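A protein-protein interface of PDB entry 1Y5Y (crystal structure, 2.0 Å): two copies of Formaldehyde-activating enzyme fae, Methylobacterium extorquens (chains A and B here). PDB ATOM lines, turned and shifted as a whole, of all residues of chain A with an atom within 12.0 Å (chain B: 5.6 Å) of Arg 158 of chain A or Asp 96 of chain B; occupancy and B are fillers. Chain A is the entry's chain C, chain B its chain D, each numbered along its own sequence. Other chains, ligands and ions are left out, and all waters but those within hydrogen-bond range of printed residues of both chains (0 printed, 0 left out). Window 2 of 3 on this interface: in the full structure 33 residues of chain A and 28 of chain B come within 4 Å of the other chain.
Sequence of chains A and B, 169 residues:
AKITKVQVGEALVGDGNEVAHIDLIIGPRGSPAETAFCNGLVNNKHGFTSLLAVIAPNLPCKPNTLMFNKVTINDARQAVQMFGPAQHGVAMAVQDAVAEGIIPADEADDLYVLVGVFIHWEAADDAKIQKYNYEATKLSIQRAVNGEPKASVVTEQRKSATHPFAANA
The side-chain hydroxyl (OG1) of Thr 155 of chain A lies within hydrogen-bond range of the side-chain amide nitrogen (NE2) of Gln 95 of chain B, at 3.0 Å. NH1 of Arg 158 of chain A is in hydrogen-bond range of SD of Met 92 of chain B (3.5 Å). OD1 of Asp 96 of chain B lies within salt-bridge range of NH2 of Arg 158 of chain A (2.5 Å).
The side-chain hydroxyl (OG1) of Thr 155 of chain A sits at hydrogen-bond distance from the backbone carbonyl oxygen (O) of Ala 151 of chain A, 2.8 Å away. ND1 of His 88 of chain B sits close to O of Ile 55 of chain B (3.3 Å). NE2 of His 88 of chain B lies within hydrogen-bond range of SD of Met 92 of chain B, at 3.5 Å. OD1 of Asp 96 of chain B lies within hydrogen-bond range of OH of Tyr 134 of chain B, at 2.5 Å.
Ala 151 of chain A touches Gln 95 of chain B. Val 154 of chain A touches Ile 55 of chain B (CG1 to CD1, 3.8 Å). Val 154 of chain A touches Gln 95 of chain B. Thr 155 of chain A touches Val 98 of chain B (OG1 to CG1, 3.6 Å). CB of Ala 99 of chain B touches CG2 of Thr 155 of chain A, at 3.8 Å. Arg 158 of chain A touches Ile 55 of chain B (CB to CD1, 3.9 Å). Arg 158 of chain A touches Gln 95 of chain B (CG to CG, 3.7 Å).
Printed residues of chain B within 4 Å of Arg 158 of chain A: Ile 55 (3.9 Å), Met 92 (3.5 Å), Gln 95 (3.7 Å) and Asp 96 (2.5 Å). Asp 96 of chain B touches one residue of chain A. No residue of chain A comes within 4 Å of Ala 93 of chain B. Of chain A, only Ala 151, Val 154, Thr 155 and Arg 158 come within 4 Å of Gln 95 of chain B. No residue of chain A comes within 4 Å of Ala 97 of chain B. Val 98 of chain B touches just one residue of chain A: Thr 155 (3.6 Å). Ala 99 of chain B touches just one residue of chain A: Thr 155. No residue of chain A comes within 4 Å of Glu 100 of chain B. No residue of chain A comes within 4 Å of Gly 101 of chain B. Of the printed residues of chain A, Ile 55 of chain B touches Val 154 and Arg 158. Printed residues of chain A within 4 Å of Met 92 of chain B: Arg 158. Val 153 of chain A touches none of the printed residues of chain B. Lys 150 of chain A touches none of the printed residues of chain B.
No position is printed for both chains. Of the 10 pairs that touch across the chains among the printed residues, none has its exchanged pair printed and touching as well.
Of the 10 printed residues of chain A, 4 touch a printed residue of chain B. Printed residues of chain A that touch a printed residue of chain B: Ala 151, Val 154, Thr 155 and Arg 158. Hydrophobic or aromatic side chains of chain A that line the printed part of chain B: Val 154. Printed residues of chain B that touch a printed residue of chain A: Ile 55, Met 92, Gln 95, Asp 96, Val 98 and Ala 99. Hydrophobic or aromatic side chains of chain B that line the printed part of chain A: Ile 55, Met 92, Val 98 and Ala 99. Among the printed residues, 10 pairs touch across the chains.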
ATOM      1  N   PRO A 149      37.467  -2.704  -0.136  1.00  0.00           N
ATOM      2  CA  PRO A 149      37.165  -3.378   1.139  1.00  0.00           C
ATOM      3  C   PRO A 149      36.529  -4.730   0.887  1.00  0.00           C
ATOM      4  O   PRO A 149      35.794  -4.913  -0.096  1.00  0.00           O
ATOM      5  CB  PRO A 149      36.186  -2.423   1.803  1.00  0.00           C
ATOM      6  CG  PRO A 149      35.363  -1.957   0.613  1.00  0.00           C
ATOM      7  CD  PRO A 149      36.511  -1.599  -0.360  1.00  0.00           C
ATOM      8  N   LYS A 150      36.833  -5.698   1.746  1.00  0.00           N
ATOM      9  CA  LYS A 150      36.247  -7.034   1.636  1.00  0.00           C
ATOM     10  C   LYS A 150      34.788  -6.908   2.087  1.00  0.00           C
ATOM     11  O   LYS A 150      34.475  -6.109   2.970  1.00  0.00           O
ATOM     12  CB  LYS A 150      36.985  -8.014   2.553  1.00  0.00           C
ATOM     13  CG  LYS A 150      38.341  -8.386   2.032  1.00  0.00           C
ATOM     14  CD  LYS A 150      38.189  -9.085   0.689  1.00  0.00           C
ATOM     15  CE  LYS A 150      39.532  -9.489   0.077  1.00  0.00           C
ATOM     16  NZ  LYS A 150      39.300 -10.216  -1.215  1.00  0.00           N
ATOM     17  N   ALA A 151      33.900  -7.674   1.475  1.00  0.00           N
ATOM     18  CA  ALA A 151      32.471  -7.600   1.828  1.00  0.00           C
ATOM     19  C   ALA A 151      32.223  -7.770   3.340  1.00  0.00           C
ATOM     20  O   ALA A 151      31.437  -7.020   3.945  1.00  0.00           O
ATOM     21  CB  ALA A 151      31.683  -8.664   1.021  1.00  0.00           C
ATOM     22  N   SER A 152      32.889  -8.750   3.957  1.00  0.00           N
ATOM     23  CA  SER A 152      32.726  -8.955   5.407  1.00  0.00           C
ATOM     24  C   SER A 152      33.071  -7.678   6.173  1.00  0.00           C
ATOM     25  O   SER A 152      32.360  -7.285   7.116  1.00  0.00           O
ATOM     26  CB  SER A 152      33.619 -10.090   5.886  1.00  0.00           C
ATOM     27  OG  SER A 152      34.982  -9.776   5.664  1.00  0.00           O
ATOM     28  N   VAL A 153      34.152  -7.012   5.766  1.00  0.00           N
ATOM     29  CA  VAL A 153      34.527  -5.762   6.426  1.00  0.00           C
ATOM     30  C   VAL A 153      33.483  -4.632   6.266  1.00  0.00           C
ATOM     31  O   VAL A 153      33.169  -3.912   7.234  1.00  0.00           O
ATOM     32  CB  VAL A 153      35.893  -5.250   5.915  1.00  0.00           C
ATOM     33  CG1 VAL A 153      36.118  -3.793   6.372  1.00  0.00           C
ATOM     34  CG2 VAL A 153      37.007  -6.161   6.446  1.00  0.00           C
ATOM     35  N   VAL A 154      32.965  -4.439   5.057  1.00  0.00           N
ATOM     36  CA  VAL A 154      31.964  -3.390   4.888  1.00  0.00           C
ATOM     37  C   VAL A 154      30.699  -3.790   5.647  1.00  0.00           C
ATOM     38  O   VAL A 154      30.034  -2.945   6.237  1.00  0.00           O
ATOM     39  CB  VAL A 154      31.556  -3.186   3.401  1.00  0.00           C
ATOM     40  CG1 VAL A 154      30.581  -2.006   3.284  1.00  0.00           C
ATOM     41  CG2 VAL A 154      32.795  -2.973   2.546  1.00  0.00           C
ATOM     42  N   THR A 155      30.360  -5.077   5.613  1.00  0.00           N
ATOM     43  CA  THR A 155      29.167  -5.550   6.306  1.00  0.00           C
ATOM     44  C   THR A 155      29.315  -5.254   7.793  1.00  0.00           C
ATOM     45  O   THR A 155      28.360  -4.813   8.440  1.00  0.00           O
ATOM     46  CB  THR A 155      28.964  -7.073   6.096  1.00  0.00           C
ATOM     47  OG1 THR A 155      28.788  -7.334   4.700  1.00  0.00           O
ATOM     48  CG2 THR A 155      27.742  -7.585   6.852  1.00  0.00           C
ATOM     49  N   GLU A 156      30.514  -5.471   8.333  1.00  0.00           N
ATOM     50  CA  GLU A 156      30.738  -5.226   9.752  1.00  0.00           C
ATOM     51  C   GLU A 156      30.670  -3.748  10.052  1.00  0.00           C
ATOM     52  O   GLU A 156      30.217  -3.354  11.120  1.00  0.00           O
ATOM     53  CB  GLU A 156      32.086  -5.804  10.200  1.00  0.00           C
ATOM     54  CG  GLU A 156      32.365  -5.650  11.693  1.00  0.00           C
ATOM     55  CD  GLU A 156      32.868  -4.252  12.073  1.00  0.00           C
ATOM     56  OE1 GLU A 156      32.729  -3.884  13.259  1.00  0.00           O
ATOM     57  OE2 GLU A 156      33.410  -3.526  11.197  1.00  0.00           O
ATOM     58  N   GLN A 157      31.121  -2.911   9.125  1.00  0.00           N
ATOM     59  CA  GLN A 157      31.046  -1.476   9.344  1.00  0.00           C
ATOM     60  C   GLN A 157      29.656  -0.951   8.967  1.00  0.00           C
ATOM     61  O   GLN A 157      29.442   0.257   8.871  1.00  0.00           O
ATOM     62  CB  GLN A 157      32.122  -0.769   8.532  1.00  0.00           C
ATOM     63  CG  GLN A 157      33.518  -1.013   9.080  1.00  0.00           C
ATOM     64  CD  GLN A 157      34.573  -0.230   8.342  1.00  0.00           C
ATOM     65  OE1 GLN A 157      35.137  -0.700   7.349  1.00  0.00           O
ATOM     66  NE2 GLN A 157      34.838   0.986   8.816  1.00  0.00           N
ATOM     67  N   ARG A 158      28.727  -1.883   8.756  1.00  0.00           N
ATOM     68  CA  ARG A 158      27.328  -1.600   8.398  1.00  0.00           C
ATOM     69  C   ARG A 158      26.425  -2.635   9.102  1.00  0.00           C
ATOM     70  O   ARG A 158      26.228  -2.490  10.333  1.00  0.00           O
ATOM     71  CB  ARG A 158      27.141  -1.702   6.875  1.00  0.00           C
ATOM     72  CG  ARG A 158      25.701  -1.956   6.406  1.00  0.00           C
ATOM     73  CD  ARG A 158      24.821  -0.756   6.663  1.00  0.00           C
ATOM     74  NE  ARG A 158      23.406  -1.002   6.384  1.00  0.00           N
ATOM     75  CZ  ARG A 158      22.459  -0.075   6.507  1.00  0.00           C
ATOM     76  NH1 ARG A 158      22.792   1.149   6.898  1.00  0.00           N
ATOM     77  NH2 ARG A 158      21.179  -0.362   6.257  1.00  0.00           N
ATOM     78  N   ILE B  55      28.583   3.331   0.722  1.00  0.00           N
ATOM     79  CA  ILE B  55      27.719   3.563   1.881  1.00  0.00           C
ATOM     80  C   ILE B  55      28.263   4.719   2.714  1.00  0.00           C
ATOM     81  O   ILE B  55      27.534   5.318   3.513  1.00  0.00           O
ATOM     82  CB  ILE B  55      27.550   2.330   2.825  1.00  0.00           C
ATOM     83  CG1 ILE B  55      28.891   1.833   3.326  1.00  0.00           C
ATOM     84  CG2 ILE B  55      26.845   1.233   2.132  1.00  0.00           C
ATOM     85  CD1 ILE B  55      28.753   1.034   4.620  1.00  0.00           C
ATOM     86  N   HIS B  88      22.840   6.550  -1.229  1.00  0.00           N
ATOM     87  CA  HIS B  88      22.913   5.946   0.101  1.00  0.00           C
ATOM     88  C   HIS B  88      21.868   4.828   0.239  1.00  0.00           C
ATOM     89  O   HIS B  88      22.155   3.747   0.773  1.00  0.00           O
ATOM     90  CB  HIS B  88      22.707   7.014   1.196  1.00  0.00           C
ATOM     91  CG  HIS B  88      23.124   6.556   2.554  1.00  0.00           C
ATOM     92  ND1 HIS B  88      24.415   6.151   2.828  1.00  0.00           N
ATOM     93  CD2 HIS B  88      22.418   6.369   3.697  1.00  0.00           C
ATOM     94  CE1 HIS B  88      24.485   5.725   4.081  1.00  0.00           C
ATOM     95  NE2 HIS B  88      23.288   5.849   4.628  1.00  0.00           N
ATOM     96  N   ALA B  91      23.084   1.833  -1.822  1.00  0.00           N
ATOM     97  CA  ALA B  91      24.248   1.177  -1.226  1.00  0.00           C
ATOM     98  C   ALA B  91      23.868   0.401   0.049  1.00  0.00           C
ATOM     99  O   ALA B  91      24.358  -0.701   0.273  1.00  0.00           O
ATOM    100  CB  ALA B  91      25.352   2.236  -0.889  1.00  0.00           C
ATOM    101  N   MET B  92      23.020   1.016   0.877  1.00  0.00           N
ATOM    102  CA  MET B  92      22.557   0.377   2.114  1.00  0.00           C
ATOM    103  C   MET B  92      21.828  -0.912   1.757  1.00  0.00           C
ATOM    104  O   MET B  92      22.004  -1.938   2.411  1.00  0.00           O
ATOM    105  CB  MET B  92      21.559   1.272   2.884  1.00  0.00           C
ATOM    106  CG  MET B  92      22.142   2.489   3.614  1.00  0.00           C
ATOM    107  SD  MET B  92      20.950   3.221   4.808  1.00  0.00           S
ATOM    108  CE  MET B  92      19.650   3.814   3.728  1.00  0.00           C
ATOM    109  N   ALA B  93      21.012  -0.864   0.709  1.00  0.00           N
ATOM    110  CA  ALA B  93      20.229  -2.041   0.321  1.00  0.00           C
ATOM    111  C   ALA B  93      21.146  -3.170  -0.116  1.00  0.00           C
ATOM    112  O   ALA B  93      20.941  -4.330   0.246  1.00  0.00           O
ATOM    113  CB  ALA B  93      19.213  -1.694  -0.794  1.00  0.00           C
ATOM    114  N   VAL B  94      22.179  -2.855  -0.898  1.00  0.00           N
ATOM    115  CA  VAL B  94      23.085  -3.907  -1.305  1.00  0.00           C
ATOM    116  C   VAL B  94      23.775  -4.528  -0.079  1.00  0.00           C
ATOM    117  O   VAL B  94      23.852  -5.779   0.055  1.00  0.00           O
ATOM    118  CB  VAL B  94      24.182  -3.366  -2.285  1.00  0.00           C
ATOM    119  CG1 VAL B  94      25.254  -4.471  -2.518  1.00  0.00           C
ATOM    120  CG2 VAL B  94      23.519  -2.992  -3.650  1.00  0.00           C
ATOM    121  N   GLN B  95      24.271  -3.675   0.812  1.00  0.00           N
ATOM    122  CA  GLN B  95      25.000  -4.176   1.958  1.00  0.00           C
ATOM    123  C   GLN B  95      24.107  -4.966   2.895  1.00  0.00           C
ATOM    124  O   GLN B  95      24.533  -5.981   3.448  1.00  0.00           O
ATOM    125  CB  GLN B  95      25.692  -3.045   2.725  1.00  0.00           C
ATOM    126  CG  GLN B  95      27.002  -3.582   3.369  1.00  0.00           C
ATOM    127  CD  GLN B  95      27.923  -4.150   2.285  1.00  0.00           C
ATOM    128  OE1 GLN B  95      28.142  -3.500   1.261  1.00  0.00           O
ATOM    129  NE2 GLN B  95      28.443  -5.365   2.488  1.00  0.00           N
ATOM    130  N   ASP B  96      22.881  -4.493   3.080  1.00  0.00           N
ATOM    131  CA  ASP B  96      21.934  -5.209   3.922  1.00  0.00           C
ATOM    132  C   ASP B  96      21.581  -6.548   3.275  1.00  0.00           C
ATOM    133  O   ASP B  96      21.411  -7.549   3.975  1.00  0.00           O
ATOM    134  CB  ASP B  96      20.687  -4.351   4.171  1.00  0.00           C
ATOM    135  CG  ASP B  96      20.934  -3.238   5.224  1.00  0.00           C
ATOM    136  OD1 ASP B  96      20.005  -2.440   5.476  1.00  0.00           O
ATOM    137  OD2 ASP B  96      22.057  -3.154   5.799  1.00  0.00           O
ATOM    138  N   ALA B  97      21.485  -6.590   1.942  1.00  0.00           N
ATOM    139  CA  ALA B  97      21.199  -7.862   1.275  1.00  0.00           C
ATOM    140  C   ALA B  97      22.292  -8.863   1.613  1.00  0.00           C
ATOM    141  O   ALA B  97      22.030 -10.056   1.735  1.00  0.00           O
ATOM    142  CB  ALA B  97      21.128  -7.692  -0.239  1.00  0.00           C
ATOM    143  N   VAL B  98      23.527  -8.385   1.728  1.00  0.00           N
ATOM    144  CA  VAL B  98      24.645  -9.262   2.076  1.00  0.00           C
ATOM    145  C   VAL B  98      24.542  -9.622   3.574  1.00  0.00           C
ATOM    146  O   VAL B  98      24.674 -10.772   3.923  1.00  0.00           O
ATOM    147  CB  VAL B  98      26.036  -8.588   1.844  1.00  0.00           C
ATOM    148  CG1 VAL B  98      27.176  -9.521   2.349  1.00  0.00           C
ATOM    149  CG2 VAL B  98      26.238  -8.327   0.343  1.00  0.00           C
ATOM    150  N   ALA B  99      24.274  -8.645   4.435  1.00  0.00           N
ATOM    151  CA  ALA B  99      24.178  -8.932   5.871  1.00  0.00           C
ATOM    152  C   ALA B  99      23.064  -9.946   6.132  1.00  0.00           C
ATOM    153  O   ALA B  99      23.166 -10.780   7.021  1.00  0.00           O
ATOM    154  CB  ALA B  99      23.928  -7.638   6.671  1.00  0.00           C
ATOM    155  N   GLU B 100      22.022  -9.908   5.325  1.00  0.00           N
ATOM    156  CA  GLU B 100      20.925 -10.834   5.520  1.00  0.00           C
ATOM    157  C   GLU B 100      21.092 -12.187   4.829  1.00  0.00           C
ATOM    158  O   GLU B 100      20.252 -13.066   4.983  1.00  0.00           O
ATOM    159  CB  GLU B 100      19.626 -10.169   5.077  1.00  0.00           C
ATOM    160  CG  GLU B 100      19.196  -9.053   6.021  1.00  0.00           C
ATOM    161  CD  GLU B 100      18.192  -8.093   5.386  1.00  0.00           C
ATOM    162  OE1 GLU B 100      17.267  -8.571   4.702  1.00  0.00           O
ATOM    163  OE2 GLU B 100      18.324  -6.859   5.579  1.00  0.00           O
ATOM    164  N   GLY B 101      22.159 -12.380   4.069  1.00  0.00           N
ATOM    165  CA  GLY B 101      22.311 -13.664   3.412  1.00  0.00           C
ATOM    166  C   GLY B 101      21.588 -13.768   2.076  1.00  0.00           C
ATOM    167  O   GLY B 101      21.727 -14.785   1.388  1.00  0.00           O
ATOM    168  N   ILE B 102      20.794 -12.761   1.702  1.00  0.00           N
ATOM    169  CA  ILE B 102      20.148 -12.778   0.380  1.00  0.00           C
ATOM    170  C   ILE B 102      21.270 -12.883  -0.686  1.00  0.00           C
ATOM    171  O   ILE B 102      21.186 -13.650  -1.644  1.00  0.00           O
ATOM    172  CB  ILE B 102      19.330 -11.509   0.167  1.00  0.00           C
ATOM    173  CG1 ILE B 102      18.163 -11.499   1.166  1.00  0.00           C
ATOM    174  CG2 ILE B 102      18.855 -11.455  -1.267  1.00  0.00           C
ATOM    175  CD1 ILE B 102      17.592 -10.122   1.452  1.00  0.00           C
ATOM    176  N   TYR B 134      15.995   2.606  -1.174  1.00  0.00           N
ATOM    177  CA  TYR B 134      16.530   1.470  -0.399  1.00  0.00           C
ATOM    178  C   TYR B 134      15.562   0.265  -0.561  1.00  0.00           C
ATOM    179  O   TYR B 134      15.957  -0.868  -0.899  1.00  0.00           O
ATOM    180  CB  TYR B 134      16.629   1.850   1.080  1.00  0.00           C
ATOM    181  CG  TYR B 134      16.895   0.683   1.980  1.00  0.00           C
ATOM    182  CD1 TYR B 134      18.200   0.281   2.244  1.00  0.00           C
ATOM    183  CD2 TYR B 134      15.836  -0.044   2.569  1.00  0.00           C
ATOM    184  CE1 TYR B 134      18.472  -0.803   3.062  1.00  0.00           C
ATOM    185  CE2 TYR B 134      16.098  -1.159   3.394  1.00  0.00           C
ATOM    186  CZ  TYR B 134      17.419  -1.524   3.635  1.00  0.00           C
ATOM    187  OH  TYR B 134      17.738  -2.583   4.457  1.00  0.00           O
